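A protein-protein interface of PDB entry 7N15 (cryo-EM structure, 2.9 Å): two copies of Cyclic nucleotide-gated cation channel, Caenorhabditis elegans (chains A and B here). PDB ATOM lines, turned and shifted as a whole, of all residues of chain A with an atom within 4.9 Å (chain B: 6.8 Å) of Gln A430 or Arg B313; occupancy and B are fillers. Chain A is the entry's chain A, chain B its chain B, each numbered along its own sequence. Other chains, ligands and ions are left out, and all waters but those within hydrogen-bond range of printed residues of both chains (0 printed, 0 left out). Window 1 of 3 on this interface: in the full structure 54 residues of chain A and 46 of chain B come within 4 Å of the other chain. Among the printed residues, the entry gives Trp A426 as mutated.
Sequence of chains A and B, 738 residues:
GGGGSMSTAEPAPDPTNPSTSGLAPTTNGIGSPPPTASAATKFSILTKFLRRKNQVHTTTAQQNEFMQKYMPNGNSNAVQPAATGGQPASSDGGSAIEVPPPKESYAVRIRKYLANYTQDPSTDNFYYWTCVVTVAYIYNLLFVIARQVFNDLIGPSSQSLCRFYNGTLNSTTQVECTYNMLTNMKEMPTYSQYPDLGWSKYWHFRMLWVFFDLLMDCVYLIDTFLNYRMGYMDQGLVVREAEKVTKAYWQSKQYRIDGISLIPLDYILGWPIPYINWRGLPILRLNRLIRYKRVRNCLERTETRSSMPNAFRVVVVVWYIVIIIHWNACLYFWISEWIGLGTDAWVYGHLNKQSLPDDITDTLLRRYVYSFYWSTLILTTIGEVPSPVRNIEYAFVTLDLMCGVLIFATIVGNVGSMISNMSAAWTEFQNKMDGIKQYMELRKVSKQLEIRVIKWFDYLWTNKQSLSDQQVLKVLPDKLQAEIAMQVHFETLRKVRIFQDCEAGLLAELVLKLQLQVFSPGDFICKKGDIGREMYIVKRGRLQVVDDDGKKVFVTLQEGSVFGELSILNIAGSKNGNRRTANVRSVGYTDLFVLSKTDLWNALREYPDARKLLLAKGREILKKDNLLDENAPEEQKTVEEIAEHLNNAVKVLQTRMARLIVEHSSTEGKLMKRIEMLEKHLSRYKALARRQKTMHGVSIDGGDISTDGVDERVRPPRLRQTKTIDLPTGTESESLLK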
ATOM      1  N   TRP A 426      40.069  16.427  22.214  1.00  0.00           N
ATOM      2  CA  TRP A 426      38.755  16.743  22.761  1.00  0.00           C
ATOM      3  C   TRP A 426      37.809  15.556  22.671  1.00  0.00           C
ATOM      4  O   TRP A 426      36.986  15.359  23.567  1.00  0.00           O
ATOM      5  CB  TRP A 426      38.179  17.957  22.034  1.00  0.00           C
ATOM      6  CG  TRP A 426      36.747  18.274  22.332  1.00  0.00           C
ATOM      7  CD1 TRP A 426      35.680  18.085  21.509  1.00  0.00           C
ATOM      8  CD2 TRP A 426      36.229  18.867  23.526  1.00  0.00           C
ATOM      9  NE1 TRP A 426      34.529  18.512  22.119  1.00  0.00           N
ATOM     10  CE2 TRP A 426      34.840  18.996  23.360  1.00  0.00           C
ATOM     11  CE3 TRP A 426      36.803  19.291  24.725  1.00  0.00           C
ATOM     12  CZ2 TRP A 426      34.022  19.533  24.344  1.00  0.00           C
ATOM     13  CZ3 TRP A 426      35.991  19.824  25.698  1.00  0.00           C
ATOM     14  CH2 TRP A 426      34.617  19.940  25.505  1.00  0.00           C
ATOM     15  N   THR A 427      37.959  14.720  21.642  1.00  0.00           N
ATOM     16  CA  THR A 427      37.121  13.532  21.508  1.00  0.00           C
ATOM     17  C   THR A 427      37.484  12.478  22.550  1.00  0.00           C
ATOM     18  O   THR A 427      36.594  11.877  23.162  1.00  0.00           O
ATOM     19  CB  THR A 427      37.243  12.978  20.088  1.00  0.00           C
ATOM     20  OG1 THR A 427      36.784  13.966  19.160  1.00  0.00           O
ATOM     21  CG2 THR A 427      36.407  11.724  19.898  1.00  0.00           C
ATOM     22  N   GLU A 428      38.784  12.278  22.804  1.00  0.00           N
ATOM     23  CA  GLU A 428      39.208  11.328  23.834  1.00  0.00           C
ATOM     24  C   GLU A 428      38.846  11.821  25.232  1.00  0.00           C
ATOM     25  O   GLU A 428      38.404  11.032  26.081  1.00  0.00           O
ATOM     26  CB  GLU A 428      40.712  11.082  23.723  1.00  0.00           C
ATOM     27  CG  GLU A 428      41.275  10.073  24.720  1.00  0.00           C
ATOM     28  CD  GLU A 428      40.811   8.650  24.462  1.00  0.00           C
ATOM     29  OE1 GLU A 428      40.536   8.307  23.293  1.00  0.00           O
ATOM     30  OE2 GLU A 428      40.717   7.871  25.434  1.00  0.00           O
ATOM     31  N   PHE A 429      38.997  13.131  25.463  1.00  0.00           N
ATOM     32  CA  PHE A 429      38.595  13.772  26.712  1.00  0.00           C
ATOM     33  C   PHE A 429      37.113  13.623  27.034  1.00  0.00           C
ATOM     34  O   PHE A 429      36.745  13.273  28.164  1.00  0.00           O
ATOM     35  CB  PHE A 429      38.999  15.241  26.646  1.00  0.00           C
ATOM     36  CG  PHE A 429      38.857  15.975  27.930  1.00  0.00           C
ATOM     37  CD1 PHE A 429      39.730  15.736  28.978  1.00  0.00           C
ATOM     38  CD2 PHE A 429      37.867  16.931  28.082  1.00  0.00           C
ATOM     39  CE1 PHE A 429      39.605  16.422  30.159  1.00  0.00           C
ATOM     40  CE2 PHE A 429      37.742  17.621  29.258  1.00  0.00           C
ATOM     41  CZ  PHE A 429      38.609  17.363  30.296  1.00  0.00           C
ATOM     42  N   GLN A 430      36.282  13.790  26.025  1.00  0.00           N
ATOM     43  CA  GLN A 430      34.827  13.729  26.199  1.00  0.00           C
ATOM     44  C   GLN A 430      34.360  12.279  26.196  1.00  0.00           C
ATOM     45  O   GLN A 430      33.266  12.054  26.657  1.00  0.00           O
ATOM     46  CB  GLN A 430      34.213  14.693  25.191  1.00  0.00           C
ATOM     47  CG  GLN A 430      34.295  16.140  25.619  1.00  0.00           C
ATOM     48  CD  GLN A 430      33.289  16.437  26.695  1.00  0.00           C
ATOM     49  OE1 GLN A 430      32.317  15.715  26.883  1.00  0.00           O
ATOM     50  NE2 GLN A 430      33.521  17.514  27.417  1.00  0.00           N
ATOM     51  N   ASN A 431      35.136  11.332  25.694  1.00  0.00           N
ATOM     52  CA  ASN A 431      34.805   9.911  25.799  1.00  0.00           C
ATOM     53  C   ASN A 431      35.091   9.456  27.224  1.00  0.00           C
ATOM     54  O   ASN A 431      34.294   8.708  27.813  1.00  0.00           O
ATOM     55  CB  ASN A 431      35.571   9.043  24.802  1.00  0.00           C
ATOM     56  CG  ASN A 431      35.024   9.147  23.390  1.00  0.00           C
ATOM     57  OD1 ASN A 431      35.629   8.646  22.445  1.00  0.00           O
ATOM     58  ND2 ASN A 431      33.869   9.787  23.242  1.00  0.00           N
ATOM     59  N   LYS A 432      36.209   9.923  27.796  1.00  0.00           N
ATOM     60  CA  LYS A 432      36.503   9.656  29.202  1.00  0.00           C
ATOM     61  C   LYS A 432      35.464  10.283  30.124  1.00  0.00           C
ATOM     62  O   LYS A 432      34.986   9.628  31.057  1.00  0.00           O
ATOM     63  CB  LYS A 432      37.894  10.169  29.562  1.00  0.00           C
ATOM     64  CG  LYS A 432      39.026   9.418  28.905  1.00  0.00           C
ATOM     65  CD  LYS A 432      40.324  10.183  29.051  1.00  0.00           C
ATOM     66  CE  LYS A 432      41.492   9.409  28.476  1.00  0.00           C
ATOM     67  NZ  LYS A 432      42.761  10.174  28.586  1.00  0.00           N
ATOM     68  N   MET A 433      35.059  11.525  29.844  1.00  0.00           N
ATOM     69  CA  MET A 433      34.080  12.175  30.710  1.00  0.00           C
ATOM     70  C   MET A 433      32.682  11.599  30.523  1.00  0.00           C
ATOM     71  O   MET A 433      31.887  11.599  31.466  1.00  0.00           O
ATOM     72  CB  MET A 433      34.068  13.678  30.477  1.00  0.00           C
ATOM     73  CG  MET A 433      33.646  14.436  31.716  1.00  0.00           C
ATOM     74  SD  MET A 433      33.114  16.103  31.378  1.00  0.00           S
ATOM     75  CE  MET A 433      34.477  16.627  30.369  1.00  0.00           C
ATOM     76  N   ASP A 434      32.368  11.082  29.329  1.00  0.00           N
ATOM     77  CA  ASP A 434      31.115  10.361  29.134  1.00  0.00           C
ATOM     78  C   ASP A 434      31.096   9.058  29.912  1.00  0.00           C
ATOM     79  O   ASP A 434      30.049   8.685  30.452  1.00  0.00           O
ATOM     80  CB  ASP A 434      30.883  10.068  27.655  1.00  0.00           C
ATOM     81  CG  ASP A 434      30.368  11.259  26.897  1.00  0.00           C
ATOM     82  OD1 ASP A 434      30.234  11.156  25.661  1.00  0.00           O
ATOM     83  OD2 ASP A 434      30.121  12.305  27.526  1.00  0.00           O
ATOM     84  N   LYS A 437      30.605  10.148  33.599  1.00  0.00           N
ATOM     85  CA  LYS A 437      29.250  10.639  33.819  1.00  0.00           C
ATOM     86  C   LYS A 437      28.217   9.526  33.742  1.00  0.00           C
ATOM     87  O   LYS A 437      27.234   9.554  34.487  1.00  0.00           O
ATOM     88  CB  LYS A 437      28.920  11.742  32.813  1.00  0.00           C
ATOM     89  CG  LYS A 437      29.472  13.105  33.189  1.00  0.00           C
ATOM     90  CD  LYS A 437      28.879  14.214  32.340  1.00  0.00           C
ATOM     91  CE  LYS A 437      29.538  14.284  30.986  1.00  0.00           C
ATOM     92  NZ  LYS A 437      29.123  15.491  30.238  1.00  0.00           N
ATOM     93  N   GLU B 300      32.146  24.234  24.665  1.00  0.00           N
ATOM     94  CA  GLU B 300      32.959  23.247  25.372  1.00  0.00           C
ATOM     95  C   GLU B 300      32.526  23.096  26.826  1.00  0.00           C
ATOM     96  O   GLU B 300      32.448  21.973  27.341  1.00  0.00           O
ATOM     97  CB  GLU B 300      34.431  23.635  25.291  1.00  0.00           C
ATOM     98  CG  GLU B 300      35.058  23.367  23.945  1.00  0.00           C
ATOM     99  CD  GLU B 300      36.497  23.807  23.881  1.00  0.00           C
ATOM    100  OE1 GLU B 300      36.946  24.507  24.809  1.00  0.00           O
ATOM    101  OE2 GLU B 300      37.181  23.452  22.900  1.00  0.00           O
ATOM    102  N   THR B 302      29.530  23.751  27.909  1.00  0.00           N
ATOM    103  CA  THR B 302      28.199  23.162  27.894  1.00  0.00           C
ATOM    104  C   THR B 302      28.267  21.663  27.652  1.00  0.00           C
ATOM    105  O   THR B 302      27.485  20.909  28.232  1.00  0.00           O
ATOM    106  CB  THR B 302      27.337  23.847  26.837  1.00  0.00           C
ATOM    107  OG1 THR B 302      27.494  25.264  26.943  1.00  0.00           O
ATOM    108  CG2 THR B 302      25.875  23.512  27.022  1.00  0.00           C
ATOM    109  N   GLU B 303      29.208  21.205  26.824  1.00  0.00           N
ATOM    110  CA  GLU B 303      29.369  19.767  26.636  1.00  0.00           C
ATOM    111  C   GLU B 303      30.005  19.105  27.849  1.00  0.00           C
ATOM    112  O   GLU B 303      29.775  17.916  28.089  1.00  0.00           O
ATOM    113  CB  GLU B 303      30.205  19.480  25.395  1.00  0.00           C
ATOM    114  CG  GLU B 303      29.886  18.148  24.759  1.00  0.00           C
ATOM    115  CD  GLU B 303      30.776  17.838  23.587  1.00  0.00           C
ATOM    116  OE1 GLU B 303      31.233  16.685  23.485  1.00  0.00           O
ATOM    117  OE2 GLU B 303      31.027  18.747  22.774  1.00  0.00           O
ATOM    118  N   THR B 304      30.812  19.848  28.608  1.00  0.00           N
ATOM    119  CA  THR B 304      31.374  19.320  29.848  1.00  0.00           C
ATOM    120  C   THR B 304      30.297  19.125  30.910  1.00  0.00           C
ATOM    121  O   THR B 304      30.191  18.052  31.512  1.00  0.00           O
ATOM    122  CB  THR B 304      32.466  20.261  30.361  1.00  0.00           C
ATOM    123  OG1 THR B 304      33.518  20.347  29.394  1.00  0.00           O
ATOM    124  CG2 THR B 304      33.025  19.785  31.677  1.00  0.00           C
ATOM    125  N   ARG B 305      29.473  20.142  31.133  1.00  0.00           N
ATOM    126  CA  ARG B 305      28.507  20.154  32.219  1.00  0.00           C
ATOM    127  C   ARG B 305      27.231  19.382  31.923  1.00  0.00           C
ATOM    128  O   ARG B 305      26.384  19.266  32.815  1.00  0.00           O
ATOM    129  CB  ARG B 305      28.131  21.595  32.562  1.00  0.00           C
ATOM    130  CG  ARG B 305      29.252  22.412  33.152  1.00  0.00           C
ATOM    131  CD  ARG B 305      28.936  23.880  33.031  1.00  0.00           C
ATOM    132  NE  ARG B 305      27.587  24.161  33.499  1.00  0.00           N
ATOM    133  CZ  ARG B 305      27.310  24.841  34.604  1.00  0.00           C
ATOM    134  NH1 ARG B 305      28.293  25.316  35.352  1.00  0.00           N
ATOM    135  NH2 ARG B 305      26.051  25.048  34.958  1.00  0.00           N
ATOM    136  N   MET B 308      23.235  15.095  29.337  1.00  0.00           N
ATOM    137  CA  MET B 308      22.932  14.435  28.069  1.00  0.00           C
ATOM    138  C   MET B 308      23.935  14.954  27.050  1.00  0.00           C
ATOM    139  O   MET B 308      23.657  15.924  26.336  1.00  0.00           O
ATOM    140  CB  MET B 308      21.499  14.716  27.619  1.00  0.00           C
ATOM    141  CG  MET B 308      20.446  14.474  28.682  1.00  0.00           C
ATOM    142  SD  MET B 308      18.771  14.643  28.051  1.00  0.00           S
ATOM    143  CE  MET B 308      18.747  13.340  26.824  1.00  0.00           C
ATOM    144  N   PRO B 309      25.121  14.348  26.970  1.00  0.00           N
ATOM    145  CA  PRO B 309      26.160  14.902  26.090  1.00  0.00           C
ATOM    146  C   PRO B 309      25.936  14.613  24.621  1.00  0.00           C
ATOM    147  O   PRO B 309      26.240  15.467  23.780  1.00  0.00           O
ATOM    148  CB  PRO B 309      27.444  14.230  26.599  1.00  0.00           C
ATOM    149  CG  PRO B 309      27.066  13.543  27.874  1.00  0.00           C
ATOM    150  CD  PRO B 309      25.630  13.216  27.753  1.00  0.00           C
ATOM    151  N   ASN B 310      25.410  13.435  24.281  1.00  0.00           N
ATOM    152  CA  ASN B 310      25.234  13.079  22.878  1.00  0.00           C
ATOM    153  C   ASN B 310      24.051  13.812  22.263  1.00  0.00           C
ATOM    154  O   ASN B 310      24.066  14.128  21.067  1.00  0.00           O
ATOM    155  CB  ASN B 310      25.068  11.572  22.739  1.00  0.00           C
ATOM    156  CG  ASN B 310      26.267  10.807  23.248  1.00  0.00           C
ATOM    157  OD1 ASN B 310      27.312  10.772  22.603  1.00  0.00           O
ATOM    158  ND2 ASN B 310      26.119  10.182  24.406  1.00  0.00           N
ATOM    159  N   ALA B 311      23.030  14.113  23.070  1.00  0.00           N
ATOM    160  CA  ALA B 311      21.924  14.942  22.599  1.00  0.00           C
ATOM    161  C   ALA B 311      22.383  16.368  22.328  1.00  0.00           C
ATOM    162  O   ALA B 311      21.972  16.979  21.335  1.00  0.00           O
ATOM    163  CB  ALA B 311      20.790  14.932  23.619  1.00  0.00           C
ATOM    164  N   PHE B 312      23.267  16.893  23.180  1.00  0.00           N
ATOM    165  CA  PHE B 312      23.852  18.206  22.941  1.00  0.00           C
ATOM    166  C   PHE B 312      24.747  18.206  21.712  1.00  0.00           C
ATOM    167  O   PHE B 312      24.754  19.184  20.959  1.00  0.00           O
ATOM    168  CB  PHE B 312      24.639  18.662  24.166  1.00  0.00           C
ATOM    169  CG  PHE B 312      25.364  19.956  23.967  1.00  0.00           C
ATOM    170  CD1 PHE B 312      24.662  21.143  23.841  1.00  0.00           C
ATOM    171  CD2 PHE B 312      26.748  19.985  23.896  1.00  0.00           C
ATOM    172  CE1 PHE B 312      25.324  22.332  23.645  1.00  0.00           C
ATOM    173  CE2 PHE B 312      27.415  21.172  23.700  1.00  0.00           C
ATOM    174  CZ  PHE B 312      26.703  22.345  23.584  1.00  0.00           C
ATOM    175  N   ARG B 313      25.477  17.109  21.479  1.00  0.00           N
ATOM    176  CA  ARG B 313      26.334  17.005  20.303  1.00  0.00           C
ATOM    177  C   ARG B 313      25.524  16.958  19.014  1.00  0.00           C
ATOM    178  O   ARG B 313      25.900  17.595  18.021  1.00  0.00           O
ATOM    179  CB  ARG B 313      27.219  15.767  20.408  1.00  0.00           C
ATOM    180  CG  ARG B 313      28.419  15.945  21.290  1.00  0.00           C
ATOM    181  CD  ARG B 313      29.015  14.612  21.663  1.00  0.00           C
ATOM    182  NE  ARG B 313      29.688  14.683  22.953  1.00  0.00           N
ATOM    183  CZ  ARG B 313      29.972  13.627  23.704  1.00  0.00           C
ATOM    184  NH1 ARG B 313      29.642  12.413  23.294  1.00  0.00           N
ATOM    185  NH2 ARG B 313      30.583  13.787  24.864  1.00  0.00           N
ATOM    186  N   VAL B 314      24.396  16.237  19.012  1.00  0.00           N
ATOM    187  CA  VAL B 314      23.608  16.203  17.783  1.00  0.00           C
ATOM    188  C   VAL B 314      22.839  17.506  17.585  1.00  0.00           C
ATOM    189  O   VAL B 314      22.630  17.918  16.440  1.00  0.00           O
ATOM    190  CB  VAL B 314      22.694  14.958  17.703  1.00  0.00           C
ATOM    191  CG1 VAL B 314      23.520  13.689  17.812  1.00  0.00           C
ATOM    192  CG2 VAL B 314      21.598  14.971  18.738  1.00  0.00           C
ATOM    193  N   VAL B 315      22.491  18.220  18.665  1.00  0.00           N
ATOM    194  CA  VAL B 315      21.874  19.541  18.516  1.00  0.00           C
ATOM    195  C   VAL B 315      22.880  20.550  17.955  1.00  0.00           C
ATOM    196  O   VAL B 315      22.548  21.345  17.061  1.00  0.00           O
ATOM    197  CB  VAL B 315      21.266  19.986  19.863  1.00  0.00           C
ATOM    198  CG1 VAL B 315      21.019  21.482  19.926  1.00  0.00           C
ATOM    199  CG2 VAL B 315      19.956  19.276  20.091  1.00  0.00           C
ATOM    200  N   VAL B 316      24.138  20.467  18.395  1.00  0.00           N
ATOM    201  CA  VAL B 316      25.182  21.368  17.908  1.00  0.00           C
ATOM    202  C   VAL B 316      25.523  21.082  16.446  1.00  0.00           C
ATOM    203  O   VAL B 316      25.684  22.012  15.648  1.00  0.00           O
ATOM    204  CB  VAL B 316      26.407  21.282  18.839  1.00  0.00           C
ATOM    205  CG1 VAL B 316      27.664  21.841  18.210  1.00  0.00           C
ATOM    206  CG2 VAL B 316      26.123  22.073  20.060  1.00  0.00           C
ATOM    207  N   VAL B 317      25.553  19.809  16.047  1.00  0.00           N
ATOM    208  CA  VAL B 317      25.889  19.542  14.649  1.00  0.00           C
ATOM    209  C   VAL B 317      24.685  19.787  13.719  1.00  0.00           C
ATOM    210  O   VAL B 317      24.876  20.138  12.549  1.00  0.00           O
ATOM    211  CB  VAL B 317      26.488  18.129  14.507  1.00  0.00           C
ATOM    212  CG1 VAL B 317      25.450  17.060  14.671  1.00  0.00           C
ATOM    213  CG2 VAL B 317      27.267  17.978  13.203  1.00  0.00           C
ATOM    214  N   VAL B 318      23.445  19.706  14.224  1.00  0.00           N
ATOM    215  CA  VAL B 318      22.290  20.131  13.433  1.00  0.00           C
ATOM    216  C   VAL B 318      22.293  21.646  13.248  1.00  0.00           C
ATOM    217  O   VAL B 318      22.005  22.152  12.153  1.00  0.00           O
ATOM    218  CB  VAL B 318      20.993  19.603  14.081  1.00  0.00           C
ATOM    219  CG1 VAL B 318      19.755  20.331  13.603  1.00  0.00           C
ATOM    220  CG2 VAL B 318      20.824  18.143  13.731  1.00  0.00           C
ATOM    221  N   TYR B 320      25.091  23.425  13.193  1.00  0.00           N
ATOM    222  CA  TYR B 320      26.187  23.630  12.244  1.00  0.00           C
ATOM    223  C   TYR B 320      25.732  23.408  10.810  1.00  0.00           C
ATOM    224  O   TYR B 320      26.077  24.190   9.917  1.00  0.00           O
ATOM    225  CB  TYR B 320      27.342  22.678  12.549  1.00  0.00           C
ATOM    226  CG  TYR B 320      28.222  23.054  13.713  1.00  0.00           C
ATOM    227  CD1 TYR B 320      28.215  24.337  14.237  1.00  0.00           C
ATOM    228  CD2 TYR B 320      29.077  22.116  14.278  1.00  0.00           C
ATOM    229  CE1 TYR B 320      29.030  24.674  15.302  1.00  0.00           C
ATOM    230  CE2 TYR B 320      29.893  22.443  15.341  1.00  0.00           C
ATOM    231  CZ  TYR B 320      29.864  23.723  15.845  1.00  0.00           C
ATOM    232  OH  TYR B 320      30.677  24.048  16.902  1.00  0.00           O
ATOM    233  N   VAL B 415      28.559  12.755  12.683  1.00  0.00           N
ATOM    234  CA  VAL B 415      27.202  12.393  13.104  1.00  0.00           C
ATOM    235  C   VAL B 415      27.075  10.884  13.297  1.00  0.00           C
ATOM    236  O   VAL B 415      26.495  10.416  14.289  1.00  0.00           O
ATOM    237  CB  VAL B 415      26.176  12.924  12.084  1.00  0.00           C
ATOM    238  CG1 VAL B 415      24.790  12.343  12.305  1.00  0.00           C
ATOM    239  CG2 VAL B 415      26.085  14.414  12.158  1.00  0.00           C
ATOM    240  N   MET B 418      28.803   9.970  16.415  1.00  0.00           N
ATOM    241  CA  MET B 418      28.078  10.423  17.600  1.00  0.00           C
ATOM    242  C   MET B 418      26.902   9.510  17.928  1.00  0.00           C
ATOM    243  O   MET B 418      26.631   9.233  19.100  1.00  0.00           O
ATOM    244  CB  MET B 418      27.591  11.860  17.414  1.00  0.00           C
ATOM    245  CG  MET B 418      28.617  12.925  17.730  1.00  0.00           C
ATOM    246  SD  MET B 418      28.281  14.439  16.816  1.00  0.00           S
ATOM    247  CE  MET B 418      29.849  15.282  16.962  1.00  0.00           C
ATOM    248  N   ASN B 421      28.361   6.166  19.236  1.00  0.00           N
ATOM    249  CA  ASN B 421      28.801   6.127  20.629  1.00  0.00           C
ATOM    250  C   ASN B 421      27.659   6.256  21.629  1.00  0.00           C
ATOM    251  O   ASN B 421      27.914   6.247  22.836  1.00  0.00           O
ATOM    252  CB  ASN B 421      29.840   7.213  20.908  1.00  0.00           C
ATOM    253  CG  ASN B 421      31.188   6.890  20.309  1.00  0.00           C
ATOM    254  OD1 ASN B 421      31.688   7.606  19.445  1.00  0.00           O
ATOM    255  ND2 ASN B 421      31.787   5.800  20.767  1.00  0.00           N
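OG1 of Thr B304 lies within hydrogen-bond range of NE2 of Gln A430 (3.5 Å). The side-chain amide oxygen (OE1) of Gln A430 sits at hydrogen-bond distance from the guanidinium group (NH2) of Arg B313, 3.3 Å away. NH1 of Arg B313 lies within salt-bridge range of OD1 of Asp A434 (2.7 Å). The side-chain amino group of Lys A437 sits at hydrogen-bond distance from the backbone carbonyl oxygen of Glu B303, at 3.3 Å. NZ of Lys A437 is in hydrogen-bond range of O of Thr B304, at 3.1 Å. The side-chain sulfur (SD) of Met A433 lies close to the backbone carbonyl oxygen (O) of Thr B304 (3.5 Å).
OG1 of Thr B304 lies within hydrogen-bond range of O of Glu B300 (2.8 Å). The side-chain carboxylate (OE1) of Glu B303 is in salt-bridge range of the guanidinium group (NE) of Arg B313, at 2.6 Å. The side-chain amide oxygen (OD1) of Asn B310 lies within hydrogen-bond range of the guanidinium group (NH1) of Arg B313 (2.9 Å).
Among the printed residues, merely in contact across the chains: Trp A426 with Glu B300 (3.5 Å), Trp A426 with Glu B303 (3.5 Å), Gln A430 with Glu B303 (3.6 Å), Asp A434 with Pro B309 (3.3 Å) and Lys A437 with Pro B309 (3.7 Å).
Printed residues of chain B within 4 Å of Trp A426: Glu B300 and Glu B303. Gln A430 touches just these residues of chain B: Glu B303, Thr B304 and Arg B313. Lys A432 touches none of the printed residues of chain B. Of the printed residues of chain B, Asp A434 touches Pro B309 and Arg B313. Printed residues of chain A within 4 Å of Glu B300: Trp A426 (3.5 Å). Printed residues of chain A within 4 Å of Glu B303: Trp A426 (3.5 Å), Gln A430 (3.6 Å) and Lys A437 (3.3 Å). Of the printed residues of chain A, Thr B304 touches Gln A430 (3.5 Å), Met A433 (3.5 Å) and Lys A437 (3.1 Å). Ala B311 touches none of the printed residues of chain A. Of chain A, only Gln A430 (3.3 Å) and Asp A434 (2.7 Å) come within 4 Å of Arg B313. The nearest printed residue of chain A that does not touch Arg B313 is Asn A431 (5.0 Å). The nearest printed residue of chain B that does not touch Trp A426 is Thr B304 (4.1 Å).
Hydrophobic or aromatic side chains of chain B within 4 Å of the printed part of chain A: Pro B309. Printed residues of chain A that touch a printed residue of chain B: Trp A426, Gln A430, Met A433, Asp A434 and Lys A437. Hydrophobic or aromatic side chains of chain A that line the printed part of chain B: Trp A426 and Met A433. Among the printed residues, 11 pairs touch across the chains.
No position is printed for both chains. Of the 11 pairs that touch across the chains among the printed residues, none has its exchanged pair printed and touching as well.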
